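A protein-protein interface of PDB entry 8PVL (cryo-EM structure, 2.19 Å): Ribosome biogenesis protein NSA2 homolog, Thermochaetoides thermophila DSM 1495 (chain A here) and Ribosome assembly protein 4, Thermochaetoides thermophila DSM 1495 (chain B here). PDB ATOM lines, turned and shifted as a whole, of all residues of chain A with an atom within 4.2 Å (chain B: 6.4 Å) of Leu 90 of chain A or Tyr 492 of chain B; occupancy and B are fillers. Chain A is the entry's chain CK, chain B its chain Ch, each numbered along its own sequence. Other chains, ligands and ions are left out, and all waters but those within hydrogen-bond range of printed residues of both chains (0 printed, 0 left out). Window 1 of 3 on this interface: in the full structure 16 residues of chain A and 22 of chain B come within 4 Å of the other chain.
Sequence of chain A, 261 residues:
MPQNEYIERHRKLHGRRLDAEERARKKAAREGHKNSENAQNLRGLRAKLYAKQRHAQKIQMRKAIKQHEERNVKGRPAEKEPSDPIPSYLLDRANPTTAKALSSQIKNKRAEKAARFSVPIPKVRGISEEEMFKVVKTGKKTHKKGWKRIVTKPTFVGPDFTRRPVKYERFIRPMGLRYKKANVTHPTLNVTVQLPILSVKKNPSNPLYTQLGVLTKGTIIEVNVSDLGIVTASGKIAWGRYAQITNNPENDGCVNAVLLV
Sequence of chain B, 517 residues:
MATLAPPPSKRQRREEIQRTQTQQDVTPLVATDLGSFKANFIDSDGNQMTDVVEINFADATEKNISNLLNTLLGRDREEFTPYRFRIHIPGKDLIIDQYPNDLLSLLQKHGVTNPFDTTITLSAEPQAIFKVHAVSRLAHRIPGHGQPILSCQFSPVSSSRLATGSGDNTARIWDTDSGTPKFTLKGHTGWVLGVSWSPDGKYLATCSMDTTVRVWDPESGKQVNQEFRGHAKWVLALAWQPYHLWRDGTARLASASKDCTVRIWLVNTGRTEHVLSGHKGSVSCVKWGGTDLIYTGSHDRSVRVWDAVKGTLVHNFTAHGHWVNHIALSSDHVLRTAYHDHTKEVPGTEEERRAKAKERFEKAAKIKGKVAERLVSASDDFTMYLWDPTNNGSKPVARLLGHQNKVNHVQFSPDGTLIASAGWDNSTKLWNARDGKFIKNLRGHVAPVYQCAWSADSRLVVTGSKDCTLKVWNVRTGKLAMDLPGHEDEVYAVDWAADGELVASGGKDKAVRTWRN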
ATOM      1  N   ILE A  86      25.182 -14.017 -25.835  1.00  0.00           N
ATOM      2  CA  ILE A  86      25.563 -15.389 -25.508  1.00  0.00           C
ATOM      3  C   ILE A  86      25.457 -15.554 -23.998  1.00  0.00           C
ATOM      4  O   ILE A  86      25.474 -14.559 -23.257  1.00  0.00           O
ATOM      5  CB  ILE A  86      26.989 -15.719 -26.016  1.00  0.00           C
ATOM      6  CG1 ILE A  86      27.945 -14.558 -25.745  1.00  0.00           C
ATOM      7  CG2 ILE A  86      26.960 -16.079 -27.492  1.00  0.00           C
ATOM      8  CD1 ILE A  86      29.397 -14.909 -25.956  1.00  0.00           C
ATOM      9  N   PRO A  87      25.326 -16.790 -23.504  1.00  0.00           N
ATOM     10  CA  PRO A  87      25.321 -16.998 -22.050  1.00  0.00           C
ATOM     11  C   PRO A  87      26.687 -16.724 -21.437  1.00  0.00           C
ATOM     12  O   PRO A  87      27.683 -16.487 -22.121  1.00  0.00           O
ATOM     13  CB  PRO A  87      24.932 -18.470 -21.882  1.00  0.00           C
ATOM     14  CG  PRO A  87      24.424 -18.904 -23.179  1.00  0.00           C
ATOM     15  CD  PRO A  87      25.016 -18.037 -24.228  1.00  0.00           C
ATOM     16  N   SER A  88      26.710 -16.761 -20.103  1.00  0.00           N
ATOM     17  CA  SER A  88      27.928 -16.439 -19.366  1.00  0.00           C
ATOM     18  C   SER A  88      29.008 -17.497 -19.547  1.00  0.00           C
ATOM     19  O   SER A  88      30.198 -17.165 -19.543  1.00  0.00           O
ATOM     20  CB  SER A  88      27.609 -16.253 -17.884  1.00  0.00           C
ATOM     21  OG  SER A  88      27.009 -17.415 -17.345  1.00  0.00           O
ATOM     22  N   TYR A  89      28.628 -18.769 -19.707  1.00  0.00           N
ATOM     23  CA  TYR A  89      29.634 -19.807 -19.903  1.00  0.00           C
ATOM     24  C   TYR A  89      30.254 -19.759 -21.294  1.00  0.00           C
ATOM     25  O   TYR A  89      31.304 -20.371 -21.511  1.00  0.00           O
ATOM     26  CB  TYR A  89      29.046 -21.197 -19.628  1.00  0.00           C
ATOM     27  CG  TYR A  89      27.781 -21.553 -20.382  1.00  0.00           C
ATOM     28  CD1 TYR A  89      27.834 -22.042 -21.683  1.00  0.00           C
ATOM     29  CD2 TYR A  89      26.536 -21.436 -19.779  1.00  0.00           C
ATOM     30  CE1 TYR A  89      26.684 -22.378 -22.366  1.00  0.00           C
ATOM     31  CE2 TYR A  89      25.380 -21.773 -20.454  1.00  0.00           C
ATOM     32  CZ  TYR A  89      25.462 -22.243 -21.747  1.00  0.00           C
ATOM     33  OH  TYR A  89      24.316 -22.578 -22.427  1.00  0.00           O
ATOM     34  N   LEU A  90      29.633 -19.054 -22.237  1.00  0.00           N
ATOM     35  CA  LEU A  90      30.202 -18.861 -23.562  1.00  0.00           C
ATOM     36  C   LEU A  90      30.978 -17.558 -23.694  1.00  0.00           C
ATOM     37  O   LEU A  90      31.542 -17.301 -24.761  1.00  0.00           O
ATOM     38  CB  LEU A  90      29.101 -18.905 -24.627  1.00  0.00           C
ATOM     39  CG  LEU A  90      28.447 -20.265 -24.873  1.00  0.00           C
ATOM     40  CD1 LEU A  90      27.543 -20.211 -26.090  1.00  0.00           C
ATOM     41  CD2 LEU A  90      29.499 -21.347 -25.030  1.00  0.00           C
ATOM     42  N   LEU A  91      31.016 -16.738 -22.647  1.00  0.00           N
ATOM     43  CA  LEU A  91      31.780 -15.500 -22.692  1.00  0.00           C
ATOM     44  C   LEU A  91      33.274 -15.795 -22.705  1.00  0.00           C
ATOM     45  O   LEU A  91      33.731 -16.827 -22.203  1.00  0.00           O
ATOM     46  CB  LEU A  91      31.431 -14.612 -21.498  1.00  0.00           C
ATOM     47  CG  LEU A  91      30.104 -13.854 -21.561  1.00  0.00           C
ATOM     48  CD1 LEU A  91      29.821 -13.165 -20.241  1.00  0.00           C
ATOM     49  CD2 LEU A  91      30.125 -12.848 -22.693  1.00  0.00           C
ATOM     50  N   ASP A  92      34.031 -14.880 -23.316  1.00  0.00           N
ATOM     51  CA  ASP A  92      35.489 -14.886 -23.428  1.00  0.00           C
ATOM     52  C   ASP A  92      36.035 -16.075 -24.207  1.00  0.00           C
ATOM     53  O   ASP A  92      37.230 -16.378 -24.096  1.00  0.00           O
ATOM     54  CB  ASP A  92      36.172 -14.827 -22.056  1.00  0.00           C
ATOM     55  CG  ASP A  92      36.186 -13.434 -21.471  1.00  0.00           C
ATOM     56  OD1 ASP A  92      36.023 -12.464 -22.238  1.00  0.00           O
ATOM     57  OD2 ASP A  92      36.353 -13.311 -20.242  1.00  0.00           O
ATOM     58  N   ARG A  93      35.211 -16.751 -24.997  1.00  0.00           N
ATOM     59  CA  ARG A  93      35.664 -17.847 -25.840  1.00  0.00           C
ATOM     60  C   ARG A  93      35.764 -17.393 -27.291  1.00  0.00           C
ATOM     61  O   ARG A  93      35.150 -16.406 -27.703  1.00  0.00           O
ATOM     62  CB  ARG A  93      34.722 -19.048 -25.734  1.00  0.00           C
ATOM     63  CG  ARG A  93      34.486 -19.529 -24.320  1.00  0.00           C
ATOM     64  CD  ARG A  93      33.658 -20.800 -24.307  1.00  0.00           C
ATOM     65  NE  ARG A  93      33.562 -21.374 -22.970  1.00  0.00           N
ATOM     66  CZ  ARG A  93      34.487 -22.145 -22.417  1.00  0.00           C
ATOM     67  NH1 ARG A  93      35.598 -22.462 -23.061  1.00  0.00           N
ATOM     68  NH2 ARG A  93      34.293 -22.611 -21.188  1.00  0.00           N
ATOM     69  N   ASN A  95      34.535 -17.360 -30.396  1.00  0.00           N
ATOM     70  CA  ASN A  95      33.285 -17.634 -31.082  1.00  0.00           C
ATOM     71  C   ASN A  95      33.345 -17.131 -32.519  1.00  0.00           C
ATOM     72  O   ASN A  95      34.009 -16.129 -32.804  1.00  0.00           O
ATOM     73  CB  ASN A  95      32.113 -16.965 -30.354  1.00  0.00           C
ATOM     74  CG  ASN A  95      31.983 -17.426 -28.913  1.00  0.00           C
ATOM     75  OD1 ASN A  95      31.918 -16.611 -27.993  1.00  0.00           O
ATOM     76  ND2 ASN A  95      31.938 -18.736 -28.712  1.00  0.00           N
ATOM     77  N   PRO B 148      18.357 -13.465 -28.063  1.00  0.00           N
ATOM     78  CA  PRO B 148      18.433 -14.811 -27.472  1.00  0.00           C
ATOM     79  C   PRO B 148      18.216 -14.839 -25.966  1.00  0.00           C
ATOM     80  O   PRO B 148      18.578 -13.912 -25.237  1.00  0.00           O
ATOM     81  CB  PRO B 148      19.850 -15.267 -27.826  1.00  0.00           C
ATOM     82  CG  PRO B 148      20.117 -14.622 -29.106  1.00  0.00           C
ATOM     83  CD  PRO B 148      19.425 -13.285 -29.069  1.00  0.00           C
ATOM     84  N   ILE B 149      17.597 -15.923 -25.514  1.00  0.00           N
ATOM     85  CA  ILE B 149      17.361 -16.159 -24.095  1.00  0.00           C
ATOM     86  C   ILE B 149      18.626 -16.731 -23.475  1.00  0.00           C
ATOM     87  O   ILE B 149      19.155 -17.748 -23.938  1.00  0.00           O
ATOM     88  CB  ILE B 149      16.170 -17.108 -23.900  1.00  0.00           C
ATOM     89  CG1 ILE B 149      14.903 -16.476 -24.467  1.00  0.00           C
ATOM     90  CG2 ILE B 149      15.991 -17.459 -22.433  1.00  0.00           C
ATOM     91  CD1 ILE B 149      13.779 -17.447 -24.626  1.00  0.00           C
ATOM     92  N   LEU B 150      19.112 -16.083 -22.421  1.00  0.00           N
ATOM     93  CA  LEU B 150      20.377 -16.465 -21.813  1.00  0.00           C
ATOM     94  C   LEU B 150      20.229 -17.168 -20.475  1.00  0.00           C
ATOM     95  O   LEU B 150      21.095 -17.969 -20.121  1.00  0.00           O
ATOM     96  CB  LEU B 150      21.273 -15.232 -21.641  1.00  0.00           C
ATOM     97  CG  LEU B 150      21.329 -14.318 -22.867  1.00  0.00           C
ATOM     98  CD1 LEU B 150      22.162 -13.083 -22.587  1.00  0.00           C
ATOM     99  CD2 LEU B 150      21.869 -15.065 -24.076  1.00  0.00           C
ATOM    100  N   SER B 151      19.159 -16.908 -19.726  1.00  0.00           N
ATOM    101  CA  SER B 151      18.951 -17.608 -18.467  1.00  0.00           C
ATOM    102  C   SER B 151      17.469 -17.899 -18.276  1.00  0.00           C
ATOM    103  O   SER B 151      16.615 -17.170 -18.778  1.00  0.00           O
ATOM    104  CB  SER B 151      19.486 -16.796 -17.282  1.00  0.00           C
ATOM    105  OG  SER B 151      19.409 -17.537 -16.078  1.00  0.00           O
ATOM    106  N   ASN B 408      31.047 -28.676 -19.581  1.00  0.00           N
ATOM    107  CA  ASN B 408      30.350 -27.402 -19.476  1.00  0.00           C
ATOM    108  C   ASN B 408      29.515 -27.293 -18.210  1.00  0.00           C
ATOM    109  O   ASN B 408      29.529 -26.247 -17.553  1.00  0.00           O
ATOM    110  CB  ASN B 408      29.451 -27.186 -20.696  1.00  0.00           C
ATOM    111  CG  ASN B 408      29.104 -25.727 -20.909  1.00  0.00           C
ATOM    112  OD1 ASN B 408      29.961 -24.918 -21.259  1.00  0.00           O
ATOM    113  ND2 ASN B 408      27.841 -25.381 -20.694  1.00  0.00           N
ATOM    114  N   TRP B 424      31.406 -30.968 -23.838  1.00  0.00           N
ATOM    115  CA  TRP B 424      31.481 -30.481 -25.210  1.00  0.00           C
ATOM    116  C   TRP B 424      31.761 -31.585 -26.220  1.00  0.00           C
ATOM    117  O   TRP B 424      31.828 -31.300 -27.418  1.00  0.00           O
ATOM    118  CB  TRP B 424      32.551 -29.394 -25.329  1.00  0.00           C
ATOM    119  CG  TRP B 424      32.138 -28.070 -24.766  1.00  0.00           C
ATOM    120  CD1 TRP B 424      31.718 -27.813 -23.495  1.00  0.00           C
ATOM    121  CD2 TRP B 424      32.108 -26.817 -25.457  1.00  0.00           C
ATOM    122  NE1 TRP B 424      31.429 -26.481 -23.350  1.00  0.00           N
ATOM    123  CE2 TRP B 424      31.658 -25.847 -24.542  1.00  0.00           C
ATOM    124  CE3 TRP B 424      32.416 -26.421 -26.761  1.00  0.00           C
ATOM    125  CZ2 TRP B 424      31.510 -24.507 -24.887  1.00  0.00           C
ATOM    126  CZ3 TRP B 424      32.268 -25.090 -27.102  1.00  0.00           C
ATOM    127  CH2 TRP B 424      31.820 -24.149 -26.169  1.00  0.00           C
ATOM    128  N   TYR B 450      25.091 -28.234 -23.523  1.00  0.00           N
ATOM    129  CA  TYR B 450      25.356 -27.081 -22.679  1.00  0.00           C
ATOM    130  C   TYR B 450      24.780 -27.233 -21.280  1.00  0.00           C
ATOM    131  O   TYR B 450      25.459 -26.900 -20.304  1.00  0.00           O
ATOM    132  CB  TYR B 450      24.811 -25.806 -23.328  1.00  0.00           C
ATOM    133  CG  TYR B 450      25.622 -25.337 -24.512  1.00  0.00           C
ATOM    134  CD1 TYR B 450      26.993 -25.546 -24.566  1.00  0.00           C
ATOM    135  CD2 TYR B 450      25.017 -24.680 -25.573  1.00  0.00           C
ATOM    136  CE1 TYR B 450      27.737 -25.119 -25.646  1.00  0.00           C
ATOM    137  CE2 TYR B 450      25.753 -24.248 -26.656  1.00  0.00           C
ATOM    138  CZ  TYR B 450      27.110 -24.471 -26.688  1.00  0.00           C
ATOM    139  OH  TYR B 450      27.845 -24.041 -27.767  1.00  0.00           O
ATOM    140  N   GLN B 451      23.549 -27.722 -21.139  1.00  0.00           N
ATOM    141  CA  GLN B 451      22.934 -27.742 -19.819  1.00  0.00           C
ATOM    142  C   GLN B 451      22.302 -29.093 -19.520  1.00  0.00           C
ATOM    143  O   GLN B 451      21.878 -29.814 -20.423  1.00  0.00           O
ATOM    144  CB  GLN B 451      21.879 -26.635 -19.673  1.00  0.00           C
ATOM    145  CG  GLN B 451      22.459 -25.232 -19.682  1.00  0.00           C
ATOM    146  CD  GLN B 451      22.052 -24.419 -18.473  1.00  0.00           C
ATOM    147  OE1 GLN B 451      20.930 -24.528 -17.985  1.00  0.00           O
ATOM    148  NE2 GLN B 451      22.973 -23.603 -17.977  1.00  0.00           N
ATOM    149  N   GLY B 464      19.972 -30.064 -22.560  1.00  0.00           N
ATOM    150  CA  GLY B 464      19.762 -29.138 -23.654  1.00  0.00           C
ATOM    151  C   GLY B 464      21.086 -28.847 -24.340  1.00  0.00           C
ATOM    152  O   GLY B 464      22.073 -28.493 -23.681  1.00  0.00           O
ATOM    153  N   SER B 465      21.091 -29.004 -25.667  1.00  0.00           N
ATOM    154  CA  SER B 465      22.353 -28.992 -26.392  1.00  0.00           C
ATOM    155  C   SER B 465      22.359 -27.963 -27.514  1.00  0.00           C
ATOM    156  O   SER B 465      21.359 -27.302 -27.805  1.00  0.00           O
ATOM    157  CB  SER B 465      22.674 -30.375 -26.963  1.00  0.00           C
ATOM    158  OG  SER B 465      23.702 -30.293 -27.930  1.00  0.00           O
ATOM    159  N   GLU B 490      20.162 -22.878 -31.216  1.00  0.00           N
ATOM    160  CA  GLU B 490      20.844 -23.500 -30.086  1.00  0.00           C
ATOM    161  C   GLU B 490      20.106 -23.267 -28.772  1.00  0.00           C
ATOM    162  O   GLU B 490      19.542 -22.195 -28.534  1.00  0.00           O
ATOM    163  CB  GLU B 490      22.270 -22.964 -29.964  1.00  0.00           C
ATOM    164  CG  GLU B 490      23.088 -23.041 -31.235  1.00  0.00           C
ATOM    165  CD  GLU B 490      24.494 -22.509 -31.046  1.00  0.00           C
ATOM    166  OE1 GLU B 490      24.913 -22.333 -29.884  1.00  0.00           O
ATOM    167  OE2 GLU B 490      25.184 -22.270 -32.058  1.00  0.00           O
ATOM    168  N   VAL B 491      20.121 -24.285 -27.918  1.00  0.00           N
ATOM    169  CA  VAL B 491      19.516 -24.213 -26.595  1.00  0.00           C
ATOM    170  C   VAL B 491      20.569 -23.740 -25.605  1.00  0.00           C
ATOM    171  O   VAL B 491      21.651 -24.329 -25.506  1.00  0.00           O
ATOM    172  CB  VAL B 491      18.944 -25.578 -26.180  1.00  0.00           C
ATOM    173  CG1 VAL B 491      18.497 -25.547 -24.734  1.00  0.00           C
ATOM    174  CG2 VAL B 491      17.792 -25.969 -27.088  1.00  0.00           C
ATOM    175  N   TYR B 492      20.255 -22.676 -24.871  1.00  0.00           N
ATOM    176  CA  TYR B 492      21.184 -22.081 -23.920  1.00  0.00           C
ATOM    177  C   TYR B 492      20.842 -22.364 -22.467  1.00  0.00           C
ATOM    178  O   TYR B 492      21.748 -22.569 -21.660  1.00  0.00           O
ATOM    179  CB  TYR B 492      21.254 -20.565 -24.129  1.00  0.00           C
ATOM    180  CG  TYR B 492      22.016 -20.138 -25.360  1.00  0.00           C
ATOM    181  CD1 TYR B 492      23.054 -20.912 -25.862  1.00  0.00           C
ATOM    182  CD2 TYR B 492      21.713 -18.947 -26.007  1.00  0.00           C
ATOM    183  CE1 TYR B 492      23.759 -20.518 -26.982  1.00  0.00           C
ATOM    184  CE2 TYR B 492      22.412 -18.545 -27.125  1.00  0.00           C
ATOM    185  CZ  TYR B 492      23.435 -19.333 -27.608  1.00  0.00           C
ATOM    186  OH  TYR B 492      24.133 -18.936 -28.720  1.00  0.00           O
ATOM    187  N   ALA B 493      19.561 -22.379 -22.105  1.00  0.00           N
ATOM    188  CA  ALA B 493      19.145 -22.545 -20.720  1.00  0.00           C
ATOM    189  C   ALA B 493      18.051 -23.596 -20.624  1.00  0.00           C
ATOM    190  O   ALA B 493      17.103 -23.593 -21.413  1.00  0.00           O
ATOM    191  CB  ALA B 493      18.650 -21.223 -20.127  1.00  0.00           C
ATOM    192  N   VAL B 494      18.198 -24.498 -19.652  1.00  0.00           N
ATOM    193  CA  VAL B 494      17.234 -25.555 -19.366  1.00  0.00           C
ATOM    194  C   VAL B 494      16.991 -25.586 -17.863  1.00  0.00           C
ATOM    195  O   VAL B 494      17.939 -25.544 -17.073  1.00  0.00           O
ATOM    196  CB  VAL B 494      17.727 -26.934 -19.862  1.00  0.00           C
ATOM    197  CG1 VAL B 494      16.775 -28.038 -19.444  1.00  0.00           C
ATOM    198  CG2 VAL B 494      17.881 -26.948 -21.364  1.00  0.00           C
ATOM    199  N   GLY B 506      15.223 -22.342 -23.266  1.00  0.00           N
ATOM    200  CA  GLY B 506      15.358 -21.093 -23.986  1.00  0.00           C
ATOM    201  C   GLY B 506      16.722 -21.019 -24.633  1.00  0.00           C
ATOM    202  O   GLY B 506      17.680 -21.655 -24.186  1.00  0.00           O
ATOM    203  N   GLY B 507      16.800 -20.229 -25.697  1.00  0.00           N
ATOM    204  CA  GLY B 507      18.050 -20.113 -26.414  1.00  0.00           C
ATOM    205  C   GLY B 507      18.052 -19.081 -27.519  1.00  0.00           C
ATOM    206  O   GLY B 507      17.498 -17.989 -27.370  1.00  0.00           O
ATOM    207  N   LYS B 508      18.671 -19.431 -28.642  1.00  0.00           N
ATOM    208  CA  LYS B 508      18.942 -18.488 -29.715  1.00  0.00           C
ATOM    209  C   LYS B 508      17.725 -18.179 -30.580  1.00  0.00           C
ATOM    210  O   LYS B 508      17.760 -17.196 -31.328  1.00  0.00           O
ATOM    211  CB  LYS B 508      20.081 -19.030 -30.581  1.00  0.00           C
ATOM    212  CG  LYS B 508      20.939 -17.985 -31.260  1.00  0.00           C
ATOM    213  CD  LYS B 508      22.087 -18.649 -32.000  1.00  0.00           C
ATOM    214  CE  LYS B 508      22.789 -17.676 -32.927  1.00  0.00           C
ATOM    215  NZ  LYS B 508      23.800 -18.364 -33.774  1.00  0.00           N
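OH of Tyr 89 of chain A is in hydrogen-bond range of O of Tyr 492 of chain B, 2.7 Å away.
The side-chain amide oxygen (OD1) of Asn 408 of chain B is in hydrogen-bond range of the indole nitrogen (NE1) of Trp 424 of chain B, 3.0 Å away. ND2 of Asn 408 of chain B lies within hydrogen-bond range of O of Tyr 450 of chain B, 2.9 Å away. The backbone NH (N) of Tyr 450 of chain B sits at hydrogen-bond distance from the backbone carbonyl oxygen (O) of Gly 464 of chain B, at 3.0 Å. O of Gly 506 of chain B lies within hydrogen-bond range of N of Tyr 492 of chain B, at 2.9 Å. The backbone carbonyl oxygen (O) of Tyr 89 of chain A sits at hydrogen-bond distance from the guanidinium group (NE) of Arg 93 of chain A, at 2.9 Å. The backbone carbonyl oxygen of Leu 90 of chain A sits close to the side-chain amide oxygen of Asn 95 of chain A (3.3 Å).
Among the printed residues, merely in contact across the chains: Ile 86 of chain A with Leu 150 of chain B, Pro 87 of chain A with Leu 150 of chain B, Pro 87 of chain A with Tyr 492 of chain B, Tyr 89 of chain A with Asn 408 of chain B, Tyr 89 of chain A with Tyr 450 of chain B, Tyr 89 of chain A with Gln 451 of chain B, Leu 90 of chain A with Trp 424 of chain B and Leu 90 of chain A with Tyr 492 of chain B.
Of the printed residues of chain B, Ile 86 of chain A touches Leu 150. Of the printed residues of chain B, Pro 87 of chain A touches Leu 150 (3.9 Å) and Tyr 492 (3.5 Å). Ser 88 of chain A touches none of the printed residues of chain B. Of the printed residues of chain B, Tyr 89 of chain A touches Asn 408 (3.5 Å), Tyr 450 (3.4 Å), Gln 451 (3.9 Å) and Tyr 492 (2.7 Å). Leu 90 of chain A touches just these residues of chain B: Trp 424 and Tyr 492. Asn 95 of chain A touches none of the printed residues of chain B. Of the printed residues of chain A, Asn 408 of chain B touches Tyr 89. Of the printed residues of chain A, Gln 451 of chain B touches Tyr 89 (3.9 Å). Tyr 492 of chain B touches just these residues of chain A: Pro 87, Tyr 89 and Leu 90. The nearest printed residue of chain A that does not touch Gln 451 of chain B is Pro 87 of chain A (6.7 Å).
Printed residues of chain B that touch a printed residue of chain A: Leu 150, Asn 408, Trp 424, Tyr 450, Gln 451 and Tyr 492. Hydrophobic or aromatic side chains of chain B that line the printed part of chain A: Leu 150, Trp 424, Tyr 450 and Tyr 492. Hydrophobic or aromatic side chains of chain A within 4 Å of the printed part of chain B: Pro 87, Tyr 89 and Leu 90. Among the printed residues, 9 pairs touch across the chains.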
